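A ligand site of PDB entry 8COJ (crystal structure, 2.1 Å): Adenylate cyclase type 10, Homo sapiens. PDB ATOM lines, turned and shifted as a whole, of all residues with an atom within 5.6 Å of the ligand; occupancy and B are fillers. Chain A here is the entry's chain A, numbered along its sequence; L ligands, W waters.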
ATOM      1  N   PHE A  45      -4.559  15.978  35.757  1.00  0.00           N
ATOM      2  CA  PHE A  45      -5.049  17.162  35.056  1.00  0.00           C
ATOM      3  C   PHE A  45      -5.718  18.040  36.083  1.00  0.00           C
ATOM      4  O   PHE A  45      -6.684  17.607  36.717  1.00  0.00           O
ATOM      5  CB  PHE A  45      -6.023  16.777  33.951  1.00  0.00           C
ATOM      6  CG  PHE A  45      -6.455  17.918  33.085  1.00  0.00           C
ATOM      7  CD1 PHE A  45      -5.816  18.162  31.873  1.00  0.00           C
ATOM      8  CD2 PHE A  45      -7.482  18.739  33.469  1.00  0.00           C
ATOM      9  CE1 PHE A  45      -6.207  19.213  31.072  1.00  0.00           C
ATOM     10  CE2 PHE A  45      -7.900  19.797  32.655  1.00  0.00           C
ATOM     11  CZ  PHE A  45      -7.263  20.014  31.450  1.00  0.00           C
ATOM     12  N   LEU A  94       3.829  18.626  32.279  1.00  0.00           N
ATOM     13  CA  LEU A  94       4.048  18.526  30.838  1.00  0.00           C
ATOM     14  C   LEU A  94       3.745  19.844  30.128  1.00  0.00           C
ATOM     15  O   LEU A  94       4.565  20.338  29.339  1.00  0.00           O
ATOM     16  CB  LEU A  94       3.204  17.395  30.263  1.00  0.00           C
ATOM     17  CG  LEU A  94       3.500  15.982  30.777  1.00  0.00           C
ATOM     18  CD1 LEU A  94       2.676  14.951  30.005  1.00  0.00           C
ATOM     19  CD2 LEU A  94       4.983  15.672  30.686  1.00  0.00           C
ATOM     20  N   LYS A  95       2.596  20.448  30.425  1.00  0.00           N
ATOM     21  CA  LYS A  95       2.191  21.668  29.726  1.00  0.00           C
ATOM     22  C   LYS A  95       1.241  22.481  30.598  1.00  0.00           C
ATOM     23  O   LYS A  95       0.514  21.937  31.429  1.00  0.00           O
ATOM     24  CB  LYS A  95       1.492  21.356  28.392  1.00  0.00           C
ATOM     25  CG  LYS A  95       2.384  21.334  27.185  1.00  0.00           C
ATOM     26  CD  LYS A  95       1.613  20.999  25.902  1.00  0.00           C
ATOM     27  CE  LYS A  95       2.567  20.458  24.841  1.00  0.00           C
ATOM     28  NZ  LYS A  95       1.928  20.410  23.468  1.00  0.00           N
ATOM     29  N   PHE A  96       1.264  23.786  30.372  1.00  0.00           N
ATOM     30  CA  PHE A  96       0.292  24.727  30.893  1.00  0.00           C
ATOM     31  C   PHE A  96      -0.607  25.156  29.753  1.00  0.00           C
ATOM     32  O   PHE A  96      -0.137  25.329  28.622  1.00  0.00           O
ATOM     33  CB  PHE A  96       0.990  25.953  31.495  1.00  0.00           C
ATOM     34  CG  PHE A  96       1.848  25.645  32.688  1.00  0.00           C
ATOM     35  CD1 PHE A  96       3.145  25.214  32.516  1.00  0.00           C
ATOM     36  CD2 PHE A  96       1.357  25.819  33.979  1.00  0.00           C
ATOM     37  CE1 PHE A  96       3.986  24.955  33.612  1.00  0.00           C
ATOM     38  CE2 PHE A  96       2.184  25.567  35.094  1.00  0.00           C
ATOM     39  CZ  PHE A  96       3.500  25.120  34.894  1.00  0.00           C
ATOM     40  N   ALA A  97      -1.910  25.346  30.038  1.00  0.00           N
ATOM     41  CA  ALA A  97      -2.835  25.718  28.976  1.00  0.00           C
ATOM     42  C   ALA A  97      -3.891  26.713  29.420  1.00  0.00           C
ATOM     43  O   ALA A  97      -4.994  26.732  28.870  1.00  0.00           O
ATOM     44  CB  ALA A  97      -3.531  24.487  28.383  1.00  0.00           C
ATOM     45  N   ASP A  99      -6.374  27.078  31.159  1.00  0.00           N
ATOM     46  CA  ASP A  99      -7.445  26.483  31.945  1.00  0.00           C
ATOM     47  C   ASP A  99      -6.973  25.311  32.793  1.00  0.00           C
ATOM     48  O   ASP A  99      -7.767  24.823  33.617  1.00  0.00           O
ATOM     49  CB  ASP A  99      -8.581  26.010  31.032  1.00  0.00           C
ATOM     50  CG  ASP A  99      -8.098  25.018  29.978  1.00  0.00           C
ATOM     51  OD1 ASP A  99      -8.735  23.969  29.783  1.00  0.00           O
ATOM     52  OD2 ASP A  99      -7.076  25.311  29.336  1.00  0.00           O
ATOM     53  N   ALA A 100      -5.720  24.870  32.650  1.00  0.00           N
ATOM     54  CA  ALA A 100      -5.243  23.719  33.413  1.00  0.00           C
ATOM     55  C   ALA A 100      -3.749  23.498  33.218  1.00  0.00           C
ATOM     56  O   ALA A 100      -3.093  24.135  32.381  1.00  0.00           O
ATOM     57  CB  ALA A 100      -6.030  22.463  33.022  1.00  0.00           C
ATOM     58  N   LEU A 101      -3.210  22.553  33.977  1.00  0.00           N
ATOM     59  CA  LEU A 101      -1.899  21.986  33.712  1.00  0.00           C
ATOM     60  C   LEU A 101      -2.017  20.470  33.776  1.00  0.00           C
ATOM     61  O   LEU A 101      -2.856  19.927  34.513  1.00  0.00           O
ATOM     62  CB  LEU A 101      -0.846  22.468  34.690  1.00  0.00           C
ATOM     63  CG  LEU A 101      -0.977  22.153  36.179  1.00  0.00           C
ATOM     64  CD1 LEU A 101      -0.413  20.804  36.508  1.00  0.00           C
ATOM     65  CD2 LEU A 101      -0.283  23.275  36.994  1.00  0.00           C
ATOM     66  N   LEU A 102      -1.181  19.807  32.982  1.00  0.00           N
ATOM     67  CA  LEU A 102      -1.142  18.350  32.886  1.00  0.00           C
ATOM     68  C   LEU A 102       0.208  17.880  33.407  1.00  0.00           C
ATOM     69  O   LEU A 102       1.256  18.401  32.994  1.00  0.00           O
ATOM     70  CB  LEU A 102      -1.342  17.883  31.457  1.00  0.00           C
ATOM     71  CG  LEU A 102      -1.351  16.374  31.204  1.00  0.00           C
ATOM     72  CD1 LEU A 102      -2.590  15.725  31.839  1.00  0.00           C
ATOM     73  CD2 LEU A 102      -1.334  16.056  29.695  1.00  0.00           C
ATOM     74  N   PHE A 165       5.578  18.509  21.148  1.00  0.00           N
ATOM     75  CA  PHE A 165       5.306  17.177  21.677  1.00  0.00           C
ATOM     76  C   PHE A 165       3.891  17.078  22.217  1.00  0.00           C
ATOM     77  O   PHE A 165       3.251  18.064  22.585  1.00  0.00           O
ATOM     78  CB  PHE A 165       6.311  16.781  22.788  1.00  0.00           C
ATOM     79  CG  PHE A 165       6.109  17.510  24.087  1.00  0.00           C
ATOM     80  CD1 PHE A 165       6.660  18.775  24.287  1.00  0.00           C
ATOM     81  CD2 PHE A 165       5.368  16.935  25.096  1.00  0.00           C
ATOM     82  CE1 PHE A 165       6.463  19.448  25.486  1.00  0.00           C
ATOM     83  CE2 PHE A 165       5.177  17.597  26.288  1.00  0.00           C
ATOM     84  CZ  PHE A 165       5.709  18.872  26.462  1.00  0.00           C
ATOM     85  N   LEU A 166       3.426  15.840  22.281  1.00  0.00           N
ATOM     86  CA  LEU A 166       2.118  15.504  22.797  1.00  0.00           C
ATOM     87  C   LEU A 166       2.204  14.135  23.455  1.00  0.00           C
ATOM     88  O   LEU A 166       2.997  13.278  23.046  1.00  0.00           O
ATOM     89  CB  LEU A 166       1.057  15.463  21.683  1.00  0.00           C
ATOM     90  CG  LEU A 166       0.600  16.774  21.057  1.00  0.00           C
ATOM     91  CD1 LEU A 166      -0.069  16.483  19.705  1.00  0.00           C
ATOM     92  CD2 LEU A 166      -0.350  17.535  21.956  1.00  0.00           C
ATOM     93  N   VAL A 167       1.360  13.908  24.437  1.00  0.00           N
ATOM     94  CA  VAL A 167       1.109  12.554  24.947  1.00  0.00           C
ATOM     95  C   VAL A 167      -0.229  12.112  24.398  1.00  0.00           C
ATOM     96  O   VAL A 167      -1.179  12.898  24.324  1.00  0.00           O
ATOM     97  CB  VAL A 167       1.147  12.494  26.486  1.00  0.00           C
ATOM     98  CG1 VAL A 167       2.603  12.556  26.976  1.00  0.00           C
ATOM     99  CG2 VAL A 167       0.297  13.588  27.102  1.00  0.00           C
ATOM    100  N   ILE A 168      -0.318  10.827  24.019  1.00  0.00           N
ATOM    101  CA  ILE A 168      -1.490  10.280  23.335  1.00  0.00           C
ATOM    102  C   ILE A 168      -1.799   8.931  23.947  1.00  0.00           C
ATOM    103  O   ILE A 168      -0.923   8.226  24.436  1.00  0.00           O
ATOM    104  CB  ILE A 168      -1.240  10.163  21.814  1.00  0.00           C
ATOM    105  CG1 ILE A 168      -1.283  11.554  21.172  1.00  0.00           C
ATOM    106  CG2 ILE A 168      -2.230   9.242  21.144  1.00  0.00           C
ATOM    107  CD1 ILE A 168      -0.665  11.599  19.785  1.00  0.00           C
ATOM    108  N   VAL A 172      -4.618   9.242  28.400  1.00  0.00           N
ATOM    109  CA  VAL A 172      -4.856  10.660  28.143  1.00  0.00           C
ATOM    110  C   VAL A 172      -6.345  10.946  28.037  1.00  0.00           C
ATOM    111  O   VAL A 172      -6.875  11.841  28.710  1.00  0.00           O
ATOM    112  CB  VAL A 172      -4.104  11.097  26.869  1.00  0.00           C
ATOM    113  CG1 VAL A 172      -4.383  12.565  26.595  1.00  0.00           C
ATOM    114  CG2 VAL A 172      -2.584  10.865  27.028  1.00  0.00           C
ATOM    115  N   ASP A 173      -7.052  10.200  27.190  1.00  0.00           N
ATOM    116  CA  ASP A 173      -8.496  10.412  27.098  1.00  0.00           C
ATOM    117  C   ASP A 173      -9.191  10.121  28.416  1.00  0.00           C
ATOM    118  O   ASP A 173     -10.205  10.755  28.735  1.00  0.00           O
ATOM    119  CB  ASP A 173      -9.070   9.537  25.986  1.00  0.00           C
ATOM    120  CG  ASP A 173      -8.416   9.788  24.639  1.00  0.00           C
ATOM    121  OD1 ASP A 173      -8.023  10.950  24.372  1.00  0.00           O
ATOM    122  OD2 ASP A 173      -8.292   8.816  23.861  1.00  0.00           O
ATOM    123  N   VAL A 175      -8.007  10.711  31.508  1.00  0.00           N
ATOM    124  CA  VAL A 175      -7.861  11.853  32.390  1.00  0.00           C
ATOM    125  C   VAL A 175      -8.667  13.020  31.869  1.00  0.00           C
ATOM    126  O   VAL A 175      -9.084  13.895  32.646  1.00  0.00           O
ATOM    127  CB  VAL A 175      -6.375  12.213  32.603  1.00  0.00           C
ATOM    128  CG1 VAL A 175      -5.851  13.118  31.510  1.00  0.00           C
ATOM    129  CG2 VAL A 175      -6.189  12.854  33.990  1.00  0.00           C
ATOM    130  N   ARG A 176      -8.917  13.058  30.552  1.00  0.00           N
ATOM    131  CA  ARG A 176      -9.826  14.057  29.995  1.00  0.00           C
ATOM    132  C   ARG A 176     -11.188  13.947  30.648  1.00  0.00           C
ATOM    133  O   ARG A 176     -11.731  14.938  31.154  1.00  0.00           O
ATOM    134  CB  ARG A 176      -9.948  13.874  28.476  1.00  0.00           C
ATOM    135  CG  ARG A 176     -10.575  15.053  27.733  1.00  0.00           C
ATOM    136  CD  ARG A 176     -12.084  15.131  27.911  1.00  0.00           C
ATOM    137  NE  ARG A 176     -12.686  16.192  27.098  1.00  0.00           N
ATOM    138  CZ  ARG A 176     -13.270  17.285  27.583  1.00  0.00           C
ATOM    139  NH1 ARG A 176     -13.792  18.173  26.758  1.00  0.00           N
ATOM    140  NH2 ARG A 176     -13.355  17.484  28.896  1.00  0.00           N
ATOM    141  N   LEU A 177     -11.767  12.754  30.649  1.00  0.00           N
ATOM    142  CA  LEU A 177     -13.135  12.588  31.121  1.00  0.00           C
ATOM    143  C   LEU A 177     -13.235  12.645  32.638  1.00  0.00           C
ATOM    144  O   LEU A 177     -14.202  13.182  33.186  1.00  0.00           O
ATOM    145  CB  LEU A 177     -13.704  11.286  30.583  1.00  0.00           C
ATOM    146  CG  LEU A 177     -13.707  11.248  29.043  1.00  0.00           C
ATOM    147  CD1 LEU A 177     -13.964   9.845  28.520  1.00  0.00           C
ATOM    148  CD2 LEU A 177     -14.720  12.251  28.467  1.00  0.00           C
ATOM    149  N   GLN A 179     -11.496  14.574  34.377  1.00  0.00           N
ATOM    150  CA  GLN A 179     -11.492  16.016  34.623  1.00  0.00           C
ATOM    151  C   GLN A 179     -12.909  16.578  34.558  1.00  0.00           C
ATOM    152  O   GLN A 179     -13.363  17.268  35.479  1.00  0.00           O
ATOM    153  CB  GLN A 179     -10.599  16.733  33.595  1.00  0.00           C
ATOM    154  CG  GLN A 179     -10.830  18.253  33.501  1.00  0.00           C
ATOM    155  CD  GLN A 179     -11.106  18.731  32.087  1.00  0.00           C
ATOM    156  OE1 GLN A 179     -11.233  17.935  31.158  1.00  0.00           O
ATOM    157  NE2 GLN A 179     -11.203  20.046  31.910  1.00  0.00           N
ATOM    158  N   VAL A 335      -0.205  23.289  21.497  1.00  0.00           N
ATOM    159  CA  VAL A 335      -0.791  22.171  20.791  1.00  0.00           C
ATOM    160  C   VAL A 335      -1.333  21.185  21.823  1.00  0.00           C
ATOM    161  O   VAL A 335      -0.640  20.876  22.789  1.00  0.00           O
ATOM    162  CB  VAL A 335       0.218  21.466  19.877  1.00  0.00           C
ATOM    163  CG1 VAL A 335      -0.485  20.359  19.086  1.00  0.00           C
ATOM    164  CG2 VAL A 335       0.848  22.471  18.921  1.00  0.00           C
ATOM    165  N   PHE A 336      -2.556  20.700  21.596  1.00  0.00           N
ATOM    166  CA  PHE A 336      -3.213  19.784  22.520  1.00  0.00           C
ATOM    167  C   PHE A 336      -3.729  18.585  21.755  1.00  0.00           C
ATOM    168  O   PHE A 336      -3.796  18.594  20.532  1.00  0.00           O
ATOM    169  CB  PHE A 336      -4.394  20.433  23.246  1.00  0.00           C
ATOM    170  CG  PHE A 336      -4.092  21.749  23.848  1.00  0.00           C
ATOM    171  CD1 PHE A 336      -3.211  21.854  24.915  1.00  0.00           C
ATOM    172  CD2 PHE A 336      -4.725  22.901  23.358  1.00  0.00           C
ATOM    173  CE1 PHE A 336      -2.954  23.095  25.467  1.00  0.00           C
ATOM    174  CE2 PHE A 336      -4.462  24.132  23.902  1.00  0.00           C
ATOM    175  CZ  PHE A 336      -3.609  24.229  24.958  1.00  0.00           C
ATOM    176  N   MET A 337      -4.109  17.543  22.502  1.00  0.00           N
ATOM    177  CA  MET A 337      -4.788  16.405  21.904  1.00  0.00           C
ATOM    178  C   MET A 337      -5.637  15.690  22.960  1.00  0.00           C
ATOM    179  O   MET A 337      -5.157  15.404  24.068  1.00  0.00           O
ATOM    180  CB  MET A 337      -3.780  15.436  21.294  1.00  0.00           C
ATOM    181  CG  MET A 337      -4.384  14.129  20.836  1.00  0.00           C
ATOM    182  SD  MET A 337      -4.755  14.110  19.097  1.00  0.00           S
ATOM    183  CE  MET A 337      -3.349  13.304  18.443  1.00  0.00           C
ATOM    184  N   PHE A 338      -6.887  15.404  22.613  1.00  0.00           N
ATOM    185  CA  PHE A 338      -7.733  14.534  23.420  1.00  0.00           C
ATOM    186  C   PHE A 338      -8.944  14.154  22.574  1.00  0.00           C
ATOM    187  O   PHE A 338      -9.494  15.002  21.864  1.00  0.00           O
ATOM    188  CB  PHE A 338      -8.161  15.174  24.742  1.00  0.00           C
ATOM    189  CG  PHE A 338      -8.825  16.507  24.586  1.00  0.00           C
ATOM    190  CD1 PHE A 338     -10.181  16.601  24.333  1.00  0.00           C
ATOM    191  CD2 PHE A 338      -8.086  17.679  24.702  1.00  0.00           C
ATOM    192  CE1 PHE A 338     -10.794  17.830  24.194  1.00  0.00           C
ATOM    193  CE2 PHE A 338      -8.692  18.924  24.572  1.00  0.00           C
ATOM    194  CZ  PHE A 338     -10.045  19.000  24.306  1.00  0.00           C
HETATM  195  C1  LIG L   1      -1.844  16.270  25.186  1.00  0.00           C
HETATM  196  C2  LIG L   1      -1.885  18.248  26.786  1.00  0.00           C
HETATM  197  C3  LIG L   1      -0.411  18.154  26.949  1.00  0.00           C
HETATM  198  C4  LIG L   1       0.270  17.102  26.184  1.00  0.00           C
HETATM  199  C5  LIG L   1      -4.179  20.605  28.425  1.00  0.00           C
HETATM  200  C6  LIG L   1      -3.961  19.608  27.533  1.00  0.00           C
HETATM  201  C7  LIG L   1      -2.621  19.311  27.572  1.00  0.00           C
HETATM  202  C8  LIG L   1      -7.010  18.151  28.111  1.00  0.00           C
HETATM  203  C9  LIG L   1      -7.708  17.052  28.913  1.00  0.00           C
HETATM  204  C10 LIG L   1      -7.076  15.677  29.037  1.00  0.00           C
HETATM  205  C11 LIG L   1      -5.748  15.407  28.352  1.00  0.00           C
HETATM  206  C12 LIG L   1      -5.054  16.485  27.524  1.00  0.00           C
HETATM  207  C13 LIG L   1      -5.688  17.858  27.425  1.00  0.00           C
HETATM  208  C14 LIG L   1      -4.982  18.942  26.623  1.00  0.00           C
HETATM  209  C15 LIG L   1      -2.784  21.913  30.051  1.00  0.00           C
HETATM  210  F1  LIG L   1      -8.908  17.321  29.505  1.00  0.00           F
HETATM  211  N1  LIG L   1      -2.569  17.318  25.923  1.00  0.00           N
HETATM  212  N2  LIG L   1      -0.397  16.169  25.315  1.00  0.00           N
HETATM  213  N3  LIG L   1      -3.006  20.912  29.012  1.00  0.00           N
HETATM  214  N4  LIG L   1      -2.038  20.091  28.473  1.00  0.00           N
HETATM  215  N5  LIG L   1      -2.529  15.340  24.324  1.00  0.00           N
HETATM  216 CL1  LIG L   1       1.991  16.973  26.359  1.00  0.00          CL
HETATM  217  O   HOH W   1      -6.984  22.491  27.661  1.00  0.00           O
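OE1 of Gln 179 sits close to F1 of the ligand, at 2.9 Å.
Merely in contact with the ligand: Phe 45 (3.2 Å), Lys 95 (3.6 Å), Phe 96 (3.9 Å), Ala 97 (3.2 Å), Ala 100 (3.2 Å), Leu 101 (3.8 Å), Leu 102 (3.6 Å), Phe 165 (3.2 Å), Leu 166 (3.6 Å), Val 172 (3.6 Å), Val 175 (3.8 Å), Arg 176 (3.3 Å), Phe 336 (3.5 Å) and Phe 338 (3.6 Å).
Hydrophobic or aromatic side chains that line the ligand: Phe 45, Ala 97, Leu 102, Phe 165, Leu 166, Val 167, Val 172, Val 175, Phe 336, Met 337 and Phe 338.
17 residues have an atom within 4 Å of the ligand: Phe 45, Lys 95, Phe 96, Ala 97, Ala 100, Leu 101, Leu 102, Phe 165, Leu 166, Val 167, Val 172, Val 175, Arg 176, Gln 179, Phe 336, Met 337 and Phe 338.
The nearest printed residue that does not touch the ligand is Leu 94 (4.1 Å).
O of Phe 165 lies within hydrogen-bond range of NZ of Lys 95, at 2.8 Å.
O of Ala 97 sits close to OD2 of Asp 99 (2.6 Å).
NZ of Lys 95 sits at hydrogen-bond distance from O of Val 335 (2.7 Å).
O of Leu 102 sits at hydrogen-bond distance from N of Leu 94 (2.7 Å).
O of Lys 95 lies within hydrogen-bond range of N of Leu 102 (3.1 Å).
The side-chain amide oxygen of Gln 179 lies close to the backbone carbonyl oxygen of Arg 176, at 3.0 Å.
The backbone carbonyl oxygen (O) of Met 337 sits at hydrogen-bond distance from a nitrogen (N5) of the ligand (2.6 Å).
N of Val 167 lies within hydrogen-bond range of N2 of the ligand.
O of Val 167 sits at hydrogen-bond distance from N5 of the ligand (2.8 Å).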
